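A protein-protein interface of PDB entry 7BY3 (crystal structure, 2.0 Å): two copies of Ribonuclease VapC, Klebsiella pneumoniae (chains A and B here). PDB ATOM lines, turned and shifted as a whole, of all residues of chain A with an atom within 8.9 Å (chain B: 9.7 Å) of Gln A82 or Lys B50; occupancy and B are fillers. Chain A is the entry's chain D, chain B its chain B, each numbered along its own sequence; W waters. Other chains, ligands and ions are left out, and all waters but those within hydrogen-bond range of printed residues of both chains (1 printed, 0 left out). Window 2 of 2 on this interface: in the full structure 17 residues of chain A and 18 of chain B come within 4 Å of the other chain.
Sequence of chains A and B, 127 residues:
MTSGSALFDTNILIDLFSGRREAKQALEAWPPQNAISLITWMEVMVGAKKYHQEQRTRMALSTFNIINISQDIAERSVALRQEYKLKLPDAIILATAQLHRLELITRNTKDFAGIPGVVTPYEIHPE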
ATOM      1  N   GLU A  75      24.314  11.065  10.887  1.00  0.00           N
ATOM      2  CA  GLU A  75      23.570  10.152  10.019  1.00  0.00           C
ATOM      3  C   GLU A  75      24.397   9.730   8.804  1.00  0.00           C
ATOM      4  O   GLU A  75      24.383   8.565   8.407  1.00  0.00           O
ATOM      5  CB  GLU A  75      22.258  10.800   9.566  1.00  0.00           C
ATOM      6  CG  GLU A  75      21.668  10.229   8.276  1.00  0.00           C
ATOM      7  CD  GLU A  75      20.996   8.879   8.466  1.00  0.00           C
ATOM      8  OE1 GLU A  75      21.704   7.851   8.484  1.00  0.00           O
ATOM      9  OE2 GLU A  75      19.753   8.844   8.585  1.00  0.00           O
ATOM     10  N   ARG A  76      25.120  10.680   8.222  1.00  0.00           N
ATOM     11  CA  ARG A  76      25.952  10.397   7.060  1.00  0.00           C
ATOM     12  C   ARG A  76      27.116   9.484   7.427  1.00  0.00           C
ATOM     13  O   ARG A  76      27.444   8.557   6.688  1.00  0.00           O
ATOM     14  CB  ARG A  76      26.477  11.698   6.447  1.00  0.00           C
ATOM     15  CG  ARG A  76      27.307  11.498   5.194  1.00  0.00           C
ATOM     16  CD  ARG A  76      26.511  10.798   4.104  1.00  0.00           C
ATOM     17  NE  ARG A  76      25.398  11.616   3.631  1.00  0.00           N
ATOM     18  CZ  ARG A  76      25.509  12.568   2.710  1.00  0.00           C
ATOM     19  NH1 ARG A  76      26.686  12.830   2.159  1.00  0.00           N
ATOM     20  NH2 ARG A  76      24.440  13.260   2.343  1.00  0.00           N
ATOM     21  N   SER A  77      27.733   9.753   8.574  1.00  0.00           N
ATOM     22  CA  SER A  77      28.853   8.953   9.059  1.00  0.00           C
ATOM     23  C   SER A  77      28.446   7.498   9.242  1.00  0.00           C
ATOM     24  O   SER A  77      29.196   6.588   8.890  1.00  0.00           O
ATOM     25  CB  SER A  77      29.386   9.516  10.376  1.00  0.00           C
ATOM     26  OG  SER A  77      29.419  10.929  10.349  1.00  0.00           O
ATOM     27  N   VAL A  78      27.254   7.292   9.794  1.00  0.00           N
ATOM     28  CA  VAL A  78      26.700   5.955   9.986  1.00  0.00           C
ATOM     29  C   VAL A  78      26.627   5.201   8.662  1.00  0.00           C
ATOM     30  O   VAL A  78      27.053   4.048   8.565  1.00  0.00           O
ATOM     31  CB  VAL A  78      25.290   6.016  10.617  1.00  0.00           C
ATOM     32  CG1 VAL A  78      24.639   4.653  10.588  1.00  0.00           C
ATOM     33  CG2 VAL A  78      25.368   6.530  12.044  1.00  0.00           C
ATOM     34  N   ALA A  79      26.096   5.868   7.643  1.00  0.00           N
ATOM     35  CA  ALA A  79      25.972   5.284   6.315  1.00  0.00           C
ATOM     36  C   ALA A  79      27.337   5.060   5.673  1.00  0.00           C
ATOM     37  O   ALA A  79      27.625   3.972   5.176  1.00  0.00           O
ATOM     38  CB  ALA A  79      25.113   6.170   5.431  1.00  0.00           C
ATOM     39  N   LEU A  80      28.172   6.095   5.691  1.00  0.00           N
ATOM     40  CA  LEU A  80      29.498   6.031   5.085  1.00  0.00           C
ATOM     41  C   LEU A  80      30.343   4.928   5.698  1.00  0.00           C
ATOM     42  O   LEU A  80      31.131   4.282   5.008  1.00  0.00           O
ATOM     43  CB  LEU A  80      30.218   7.372   5.231  1.00  0.00           C
ATOM     44  CG  LEU A  80      29.726   8.490   4.316  1.00  0.00           C
ATOM     45  CD1 LEU A  80      30.552   9.740   4.533  1.00  0.00           C
ATOM     46  CD2 LEU A  80      29.781   8.055   2.861  1.00  0.00           C
ATOM     47  N   ARG A  81      30.172   4.719   6.998  1.00  0.00           N
ATOM     48  CA  ARG A  81      30.934   3.704   7.707  1.00  0.00           C
ATOM     49  C   ARG A  81      30.668   2.312   7.141  1.00  0.00           C
ATOM     50  O   ARG A  81      31.591   1.521   6.954  1.00  0.00           O
ATOM     51  CB  ARG A  81      30.613   3.732   9.202  1.00  0.00           C
ATOM     52  CG  ARG A  81      31.130   2.509   9.903  1.00  0.00           C
ATOM     53  CD  ARG A  81      31.216   2.636  11.407  1.00  0.00           C
ATOM     54  NE  ARG A  81      32.067   1.570  11.931  1.00  0.00           N
ATOM     55  CZ  ARG A  81      31.739   0.280  11.923  1.00  0.00           C
ATOM     56  NH1 ARG A  81      30.575  -0.118  11.433  1.00  0.00           N
ATOM     57  NH2 ARG A  81      32.576  -0.620  12.404  1.00  0.00           N
ATOM     58  N   GLN A  82      29.403   2.023   6.857  1.00  0.00           N
ATOM     59  CA  GLN A  82      29.027   0.735   6.288  1.00  0.00           C
ATOM     60  C   GLN A  82      29.458   0.603   4.830  1.00  0.00           C
ATOM     61  O   GLN A  82      29.983  -0.434   4.423  1.00  0.00           O
ATOM     62  CB  GLN A  82      27.518   0.522   6.400  1.00  0.00           C
ATOM     63  CG  GLN A  82      27.075  -0.054   7.729  1.00  0.00           C
ATOM     64  CD  GLN A  82      26.000  -1.107   7.563  1.00  0.00           C
ATOM     65  OE1 GLN A  82      25.551  -1.377   6.449  1.00  0.00           O
ATOM     66  NE2 GLN A  82      25.589  -1.715   8.669  1.00  0.00           N
ATOM     67  N   GLU A  83      29.232   1.659   4.053  1.00  0.00           N
ATOM     68  CA  GLU A  83      29.538   1.658   2.625  1.00  0.00           C
ATOM     69  C   GLU A  83      31.005   1.356   2.329  1.00  0.00           C
ATOM     70  O   GLU A  83      31.320   0.424   1.591  1.00  0.00           O
ATOM     71  CB  GLU A  83      29.163   3.008   2.008  1.00  0.00           C
ATOM     72  CG  GLU A  83      27.676   3.310   2.015  1.00  0.00           C
ATOM     73  CD  GLU A  83      27.366   4.704   1.504  1.00  0.00           C
ATOM     74  OE1 GLU A  83      28.290   5.372   0.998  1.00  0.00           O
ATOM     75  OE2 GLU A  83      26.197   5.132   1.610  1.00  0.00           O
ATOM     76  N   TYR A  84      31.897   2.161   2.898  1.00  0.00           N
ATOM     77  CA  TYR A  84      33.326   2.063   2.617  1.00  0.00           C
ATOM     78  C   TYR A  84      34.123   1.262   3.650  1.00  0.00           C
ATOM     79  O   TYR A  84      35.351   1.197   3.564  1.00  0.00           O
ATOM     80  CB  TYR A  84      33.915   3.465   2.479  1.00  0.00           C
ATOM     81  CG  TYR A  84      33.377   4.206   1.280  1.00  0.00           C
ATOM     82  CD1 TYR A  84      33.425   3.638   0.014  1.00  0.00           C
ATOM     83  CD2 TYR A  84      32.807   5.464   1.412  1.00  0.00           C
ATOM     84  CE1 TYR A  84      32.932   4.305  -1.088  1.00  0.00           C
ATOM     85  CE2 TYR A  84      32.311   6.140   0.313  1.00  0.00           C
ATOM     86  CZ  TYR A  84      32.377   5.555  -0.934  1.00  0.00           C
ATOM     87  OH  TYR A  84      31.885   6.221  -2.030  1.00  0.00           O
ATOM     88  N   LYS A  85      33.425   0.666   4.614  1.00  0.00           N
ATOM     89  CA  LYS A  85      34.054  -0.080   5.707  1.00  0.00           C
ATOM     90  C   LYS A  85      35.039   0.809   6.452  1.00  0.00           C
ATOM     91  O   LYS A  85      36.199   0.451   6.658  1.00  0.00           O
ATOM     92  CB  LYS A  85      34.748  -1.342   5.187  1.00  0.00           C
ATOM     93  CG  LYS A  85      33.861  -2.214   4.321  1.00  0.00           C
ATOM     94  CD  LYS A  85      32.605  -2.630   5.065  1.00  0.00           C
ATOM     95  CE  LYS A  85      31.669  -3.413   4.164  1.00  0.00           C
ATOM     96  NZ  LYS A  85      32.375  -4.527   3.474  1.00  0.00           N
ATOM     97  N   LEU A  86      34.553   1.978   6.848  1.00  0.00           N
ATOM     98  CA  LEU A  86      35.356   2.977   7.534  1.00  0.00           C
ATOM     99  C   LEU A  86      35.227   2.877   9.041  1.00  0.00           C
ATOM    100  O   LEU A  86      34.183   2.504   9.564  1.00  0.00           O
ATOM    101  CB  LEU A  86      34.952   4.382   7.089  1.00  0.00           C
ATOM    102  CG  LEU A  86      35.406   4.838   5.709  1.00  0.00           C
ATOM    103  CD1 LEU A  86      34.642   6.076   5.313  1.00  0.00           C
ATOM    104  CD2 LEU A  86      36.895   5.113   5.723  1.00  0.00           C
ATOM    105  N   LYS A  87      36.311   3.190   9.736  1.00  0.00           N
ATOM    106  CA  LYS A  87      36.242   3.426  11.168  1.00  0.00           C
ATOM    107  C   LYS A  87      35.420   4.685  11.423  1.00  0.00           C
ATOM    108  O   LYS A  87      35.336   5.559  10.561  1.00  0.00           O
ATOM    109  CB  LYS A  87      37.646   3.554  11.754  1.00  0.00           C
ATOM    110  CG  LYS A  87      38.400   2.234  11.778  1.00  0.00           C
ATOM    111  CD  LYS A  87      39.834   2.348  11.270  1.00  0.00           C
ATOM    112  CE  LYS A  87      40.530   3.604  11.763  1.00  0.00           C
ATOM    113  NZ  LYS A  87      40.478   3.743  13.238  1.00  0.00           N
ATOM    114  N   LEU A  88      34.812   4.773  12.601  1.00  0.00           N
ATOM    115  CA  LEU A  88      33.897   5.871  12.921  1.00  0.00           C
ATOM    116  C   LEU A  88      34.502   7.285  12.800  1.00  0.00           C
ATOM    117  O   LEU A  88      33.862   8.165  12.228  1.00  0.00           O
ATOM    118  CB  LEU A  88      33.318   5.677  14.328  1.00  0.00           C
ATOM    119  CG  LEU A  88      32.287   6.715  14.782  1.00  0.00           C
ATOM    120  CD1 LEU A  88      31.194   6.877  13.738  1.00  0.00           C
ATOM    121  CD2 LEU A  88      31.682   6.323  16.118  1.00  0.00           C
ATOM    122  N   ALA A  91      34.888   8.064   9.183  1.00  0.00           N
ATOM    123  CA  ALA A  91      33.571   8.252   8.588  1.00  0.00           C
ATOM    124  C   ALA A  91      33.038   9.646   8.891  1.00  0.00           C
ATOM    125  O   ALA A  91      32.445  10.294   8.031  1.00  0.00           O
ATOM    126  CB  ALA A  91      32.605   7.190   9.090  1.00  0.00           C
ATOM    127  N   ILE B  14      23.489  -0.954  24.040  1.00  0.00           N
ATOM    128  CA  ILE B  14      23.741  -2.180  23.291  1.00  0.00           C
ATOM    129  C   ILE B  14      23.202  -3.393  24.041  1.00  0.00           C
ATOM    130  O   ILE B  14      22.541  -4.252  23.457  1.00  0.00           O
ATOM    131  CB  ILE B  14      25.247  -2.374  23.017  1.00  0.00           C
ATOM    132  CG1 ILE B  14      25.764  -1.278  22.086  1.00  0.00           C
ATOM    133  CG2 ILE B  14      25.510  -3.739  22.402  1.00  0.00           C
ATOM    134  CD1 ILE B  14      25.090  -1.265  20.732  1.00  0.00           C
ATOM    135  N   SER B  18      20.139  -5.825  22.825  1.00  0.00           N
ATOM    136  CA  SER B  18      20.528  -7.222  22.688  1.00  0.00           C
ATOM    137  C   SER B  18      19.730  -8.107  23.640  1.00  0.00           C
ATOM    138  O   SER B  18      19.883  -9.327  23.644  1.00  0.00           O
ATOM    139  CB  SER B  18      22.028  -7.389  22.936  1.00  0.00           C
ATOM    140  OG  SER B  18      22.782  -6.668  21.977  1.00  0.00           O
ATOM    141  N   MET B  42      25.647   7.208  17.267  1.00  0.00           N
ATOM    142  CA  MET B  42      26.269   6.673  16.059  1.00  0.00           C
ATOM    143  C   MET B  42      26.676   5.207  16.203  1.00  0.00           C
ATOM    144  O   MET B  42      26.436   4.401  15.305  1.00  0.00           O
ATOM    145  CB  MET B  42      27.493   7.509  15.675  1.00  0.00           C
ATOM    146  CG  MET B  42      27.160   8.912  15.199  1.00  0.00           C
ATOM    147  SD  MET B  42      28.592   9.781  14.538  1.00  0.00           S
ATOM    148  CE  MET B  42      29.121  10.702  15.976  1.00  0.00           C
ATOM    149  N   GLU B  43      27.292   4.865  17.332  1.00  0.00           N
ATOM    150  CA  GLU B  43      27.762   3.500  17.557  1.00  0.00           C
ATOM    151  C   GLU B  43      26.613   2.516  17.741  1.00  0.00           C
ATOM    152  O   GLU B  43      26.755   1.331  17.446  1.00  0.00           O
ATOM    153  CB  GLU B  43      28.696   3.437  18.769  1.00  0.00           C
ATOM    154  CG  GLU B  43      30.034   4.128  18.564  1.00  0.00           C
ATOM    155  CD  GLU B  43      31.110   3.617  19.508  1.00  0.00           C
ATOM    156  OE1 GLU B  43      30.982   2.471  19.989  1.00  0.00           O
ATOM    157  OE2 GLU B  43      32.085   4.356  19.762  1.00  0.00           O
ATOM    158  N   VAL B  44      25.477   3.000  18.232  1.00  0.00           N
ATOM    159  CA  VAL B  44      24.292   2.158  18.347  1.00  0.00           C
ATOM    160  C   VAL B  44      23.655   1.961  16.971  1.00  0.00           C
ATOM    161  O   VAL B  44      23.205   0.865  16.635  1.00  0.00           O
ATOM    162  CB  VAL B  44      23.260   2.756  19.329  1.00  0.00           C
ATOM    163  CG1 VAL B  44      21.963   1.966  19.292  1.00  0.00           C
ATOM    164  CG2 VAL B  44      23.824   2.769  20.741  1.00  0.00           C
ATOM    165  N   MET B  45      23.644   3.022  16.169  1.00  0.00           N
ATOM    166  CA  MET B  45      23.065   2.967  14.828  1.00  0.00           C
ATOM    167  C   MET B  45      23.854   2.038  13.905  1.00  0.00           C
ATOM    168  O   MET B  45      23.304   1.495  12.947  1.00  0.00           O
ATOM    169  CB  MET B  45      22.982   4.368  14.218  1.00  0.00           C
ATOM    170  CG  MET B  45      21.911   5.254  14.837  1.00  0.00           C
ATOM    171  SD  MET B  45      20.270   4.504  14.831  1.00  0.00           S
ATOM    172  CE  MET B  45      19.970   4.364  13.074  1.00  0.00           C
ATOM    173  N   VAL B  46      25.140   1.867  14.193  1.00  0.00           N
ATOM    174  CA  VAL B  46      25.954   0.888  13.482  1.00  0.00           C
ATOM    175  C   VAL B  46      25.361  -0.503  13.688  1.00  0.00           C
ATOM    176  O   VAL B  46      25.270  -1.300  12.753  1.00  0.00           O
ATOM    177  CB  VAL B  46      27.424   0.912  13.960  1.00  0.00           C
ATOM    178  CG1 VAL B  46      28.128  -0.399  13.634  1.00  0.00           C
ATOM    179  CG2 VAL B  46      28.162   2.096  13.353  1.00  0.00           C
ATOM    180  N   GLY B  47      24.937  -0.776  14.917  1.00  0.00           N
ATOM    181  CA  GLY B  47      24.340  -2.054  15.256  1.00  0.00           C
ATOM    182  C   GLY B  47      22.904  -2.166  14.786  1.00  0.00           C
ATOM    183  O   GLY B  47      22.436  -3.254  14.453  1.00  0.00           O
ATOM    184  N   ALA B  48      22.202  -1.039  14.764  1.00  0.00           N
ATOM    185  CA  ALA B  48      20.827  -1.004  14.279  1.00  0.00           C
ATOM    186  C   ALA B  48      20.769  -1.387  12.808  1.00  0.00           C
ATOM    187  O   ALA B  48      19.818  -2.019  12.353  1.00  0.00           O
ATOM    188  CB  ALA B  48      20.227   0.371  14.492  1.00  0.00           C
ATOM    189  N   LYS B  49      21.805  -0.998  12.072  1.00  0.00           N
ATOM    190  CA  LYS B  49      21.890  -1.273  10.645  1.00  0.00           C
ATOM    191  C   LYS B  49      22.259  -2.725  10.371  1.00  0.00           C
ATOM    192  O   LYS B  49      21.669  -3.365   9.500  1.00  0.00           O
ATOM    193  CB  LYS B  49      22.906  -0.340   9.991  1.00  0.00           C
ATOM    194  CG  LYS B  49      22.412   1.082   9.865  1.00  0.00           C
ATOM    195  CD  LYS B  49      23.090   1.813   8.731  1.00  0.00           C
ATOM    196  CE  LYS B  49      22.359   3.104   8.420  1.00  0.00           C
ATOM    197  NZ  LYS B  49      23.128   3.974   7.493  1.00  0.00           N
ATOM    198  N   LYS B  50      23.237  -3.237  11.112  1.00  0.00           N
ATOM    199  CA  LYS B  50      23.660  -4.627  10.972  1.00  0.00           C
ATOM    200  C   LYS B  50      22.502  -5.591  11.215  1.00  0.00           C
ATOM    201  O   LYS B  50      22.328  -6.565  10.481  1.00  0.00           O
ATOM    202  CB  LYS B  50      24.815  -4.938  11.932  1.00  0.00           C
ATOM    203  CG  LYS B  50      25.016  -6.428  12.199  1.00  0.00           C
ATOM    204  CD  LYS B  50      26.474  -6.771  12.472  1.00  0.00           C
ATOM    205  CE  LYS B  50      26.985  -6.100  13.735  1.00  0.00           C
ATOM    206  NZ  LYS B  50      28.337  -6.600  14.112  1.00  0.00           N
ATOM    207  N   TYR B  51      21.705  -5.304  12.241  1.00  0.00           N
ATOM    208  CA  TYR B  51      20.613  -6.186  12.639  1.00  0.00           C
ATOM    209  C   TYR B  51      19.267  -5.784  12.035  1.00  0.00           C
ATOM    210  O   TYR B  51      18.243  -6.401  12.334  1.00  0.00           O
ATOM    211  CB  TYR B  51      20.508  -6.230  14.164  1.00  0.00           C
ATOM    212  CG  TYR B  51      21.671  -6.941  14.819  1.00  0.00           C
ATOM    213  CD1 TYR B  51      21.774  -8.324  14.777  1.00  0.00           C
ATOM    214  CD2 TYR B  51      22.666  -6.229  15.475  1.00  0.00           C
ATOM    215  CE1 TYR B  51      22.834  -8.978  15.370  1.00  0.00           C
ATOM    216  CE2 TYR B  51      23.730  -6.874  16.073  1.00  0.00           C
ATOM    217  CZ  TYR B  51      23.809  -8.250  16.017  1.00  0.00           C
ATOM    218  OH  TYR B  51      24.867  -8.898  16.609  1.00  0.00           O
ATOM    219  N   HIS B  52      19.278  -4.745  11.205  1.00  0.00           N
ATOM    220  CA  HIS B  52      18.113  -4.324  10.420  1.00  0.00           C
ATOM    221  C   HIS B  52      16.929  -3.858  11.274  1.00  0.00           C
ATOM    222  O   HIS B  52      15.771  -4.002  10.884  1.00  0.00           O
ATOM    223  CB  HIS B  52      17.674  -5.460   9.492  1.00  0.00           C
ATOM    224  CG  HIS B  52      18.796  -6.073   8.716  1.00  0.00           C
ATOM    225  ND1 HIS B  52      19.025  -7.431   8.675  1.00  0.00           N
ATOM    226  CD2 HIS B  52      19.763  -5.507   7.950  1.00  0.00           C
ATOM    227  CE1 HIS B  52      20.077  -7.677   7.921  1.00  0.00           C
ATOM    228  NE2 HIS B  52      20.546  -6.531   7.468  1.00  0.00           N
ATOM    229  N   GLN B  53      17.233  -3.321  12.452  1.00  0.00           N
ATOM    230  CA  GLN B  53      16.242  -2.708  13.341  1.00  0.00           C
ATOM    231  C   GLN B  53      16.168  -1.183  13.233  1.00  0.00           C
ATOM    232  O   GLN B  53      15.559  -0.525  14.074  1.00  0.00           O
ATOM    233  CB  GLN B  53      16.498  -3.124  14.784  1.00  0.00           C
ATOM    234  CG  GLN B  53      16.094  -4.558  15.019  1.00  0.00           C
ATOM    235  CD  GLN B  53      14.666  -4.827  14.567  1.00  0.00           C
ATOM    236  OE1 GLN B  53      13.760  -4.033  14.822  1.00  0.00           O
ATOM    237  NE2 GLN B  53      14.467  -5.937  13.868  1.00  0.00           N
ATOM    238  N   GLU B  54      16.814  -0.642  12.206  1.00  0.00           N
ATOM    239  CA  GLU B  54      17.144   0.779  12.086  1.00  0.00           C
ATOM    240  C   GLU B  54      16.054   1.790  12.468  1.00  0.00           C
ATOM    241  O   GLU B  54      16.312   2.705  13.251  1.00  0.00           O
ATOM    242  CB  GLU B  54      17.565   1.045  10.641  1.00  0.00           C
ATOM    243  CG  GLU B  54      18.070   2.439  10.357  1.00  0.00           C
ATOM    244  CD  GLU B  54      18.792   2.509   9.029  1.00  0.00           C
ATOM    245  OE1 GLU B  54      18.629   3.517   8.309  1.00  0.00           O
ATOM    246  OE2 GLU B  54      19.510   1.544   8.696  1.00  0.00           O
ATOM    247  N   THR B  57      15.128   1.330  16.272  1.00  0.00           N
ATOM    248  CA  THR B  57      16.194   1.778  17.161  1.00  0.00           C
ATOM    249  C   THR B  57      16.233   3.296  17.210  1.00  0.00           C
ATOM    250  O   THR B  57      16.300   3.895  18.284  1.00  0.00           O
ATOM    251  CB  THR B  57      17.563   1.254  16.715  1.00  0.00           C
ATOM    252  OG1 THR B  57      17.545  -0.179  16.699  1.00  0.00           O
ATOM    253  CG2 THR B  57      18.651   1.735  17.662  1.00  0.00           C
HETATM  254  O   HOH W   1      18.532   6.330   9.672  1.00  0.00           O
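Met B45 touches Val A78 (CB to CG2, 3.9 Å). Lys B49 touches Val A78 (CE to CG1, 3.5 Å). Lys B49 touches Ala A79. Arg A81 touches Val B46 (NH1 to CG1, 3.3 Å). Gln A82 touches Lys B49 (NE2 to CB, 3.3 Å). Gln A82 touches Lys B50 (NE2 to N, 3.7 Å). Met B42 touches Leu A88 (SD to CD1, 3.98 Å). Glu B43 touches Leu A88 (CG to CD2, 3.7 Å).
No position is printed for both chains. Of the 8 pairs that touch across the chains among the printed residues, none has its exchanged pair printed and touching as well.
N of Leu A86 is in hydrogen-bond range of O of Arg A81 (3.0 Å).
Leu A80 touches none of the printed residues of chain B. Printed residues of chain B within 4 Å of Arg A81: Val B46 (3.3 Å). Of chain B, only Lys B49 (3.3 Å) and Lys B50 (3.7 Å) come within 4 Å of Gln A82. Printed residues of chain B within 4 Å of Leu A88: Met B42 and Glu B43. Printed residues of chain A within 4 Å of Met B42: Leu A88 (3.98 Å). Printed residues of chain A within 4 Å of Glu B43: Leu A88. Printed residues of chain A within 4 Å of Val B46: Arg A81 (3.3 Å). Of chain A, only Gln A82 comes within 4 Å of Lys B50. No residue of chain A comes within 4 Å of Tyr B51. Thr B57 touches none of the printed residues of chain A. The nearest printed residue of chain B that does not touch Ala A79 is Val B46 (7.1 Å).
Water W1 bridges OE2 of Glu A75 and OE1 of Glu B54.
Of the 15 printed residues of chain A, 5 touch a printed residue of chain B. Along chain A the printed residues that touch a printed residue of chain B span positions 78 to 88. Of the 16 printed residues of chain B, 6 touch a printed residue of chain A. Hydrophobic or aromatic side chains of chain B that line the printed part of chain A: Met B42, Met B45 and Val B46. Among the printed residues, 8 pairs touch across the chains. Among the printed residues, no Asp or Glu carboxylate lies within 4 Å of a Lys or Arg side-chain nitrogen of the other chain.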
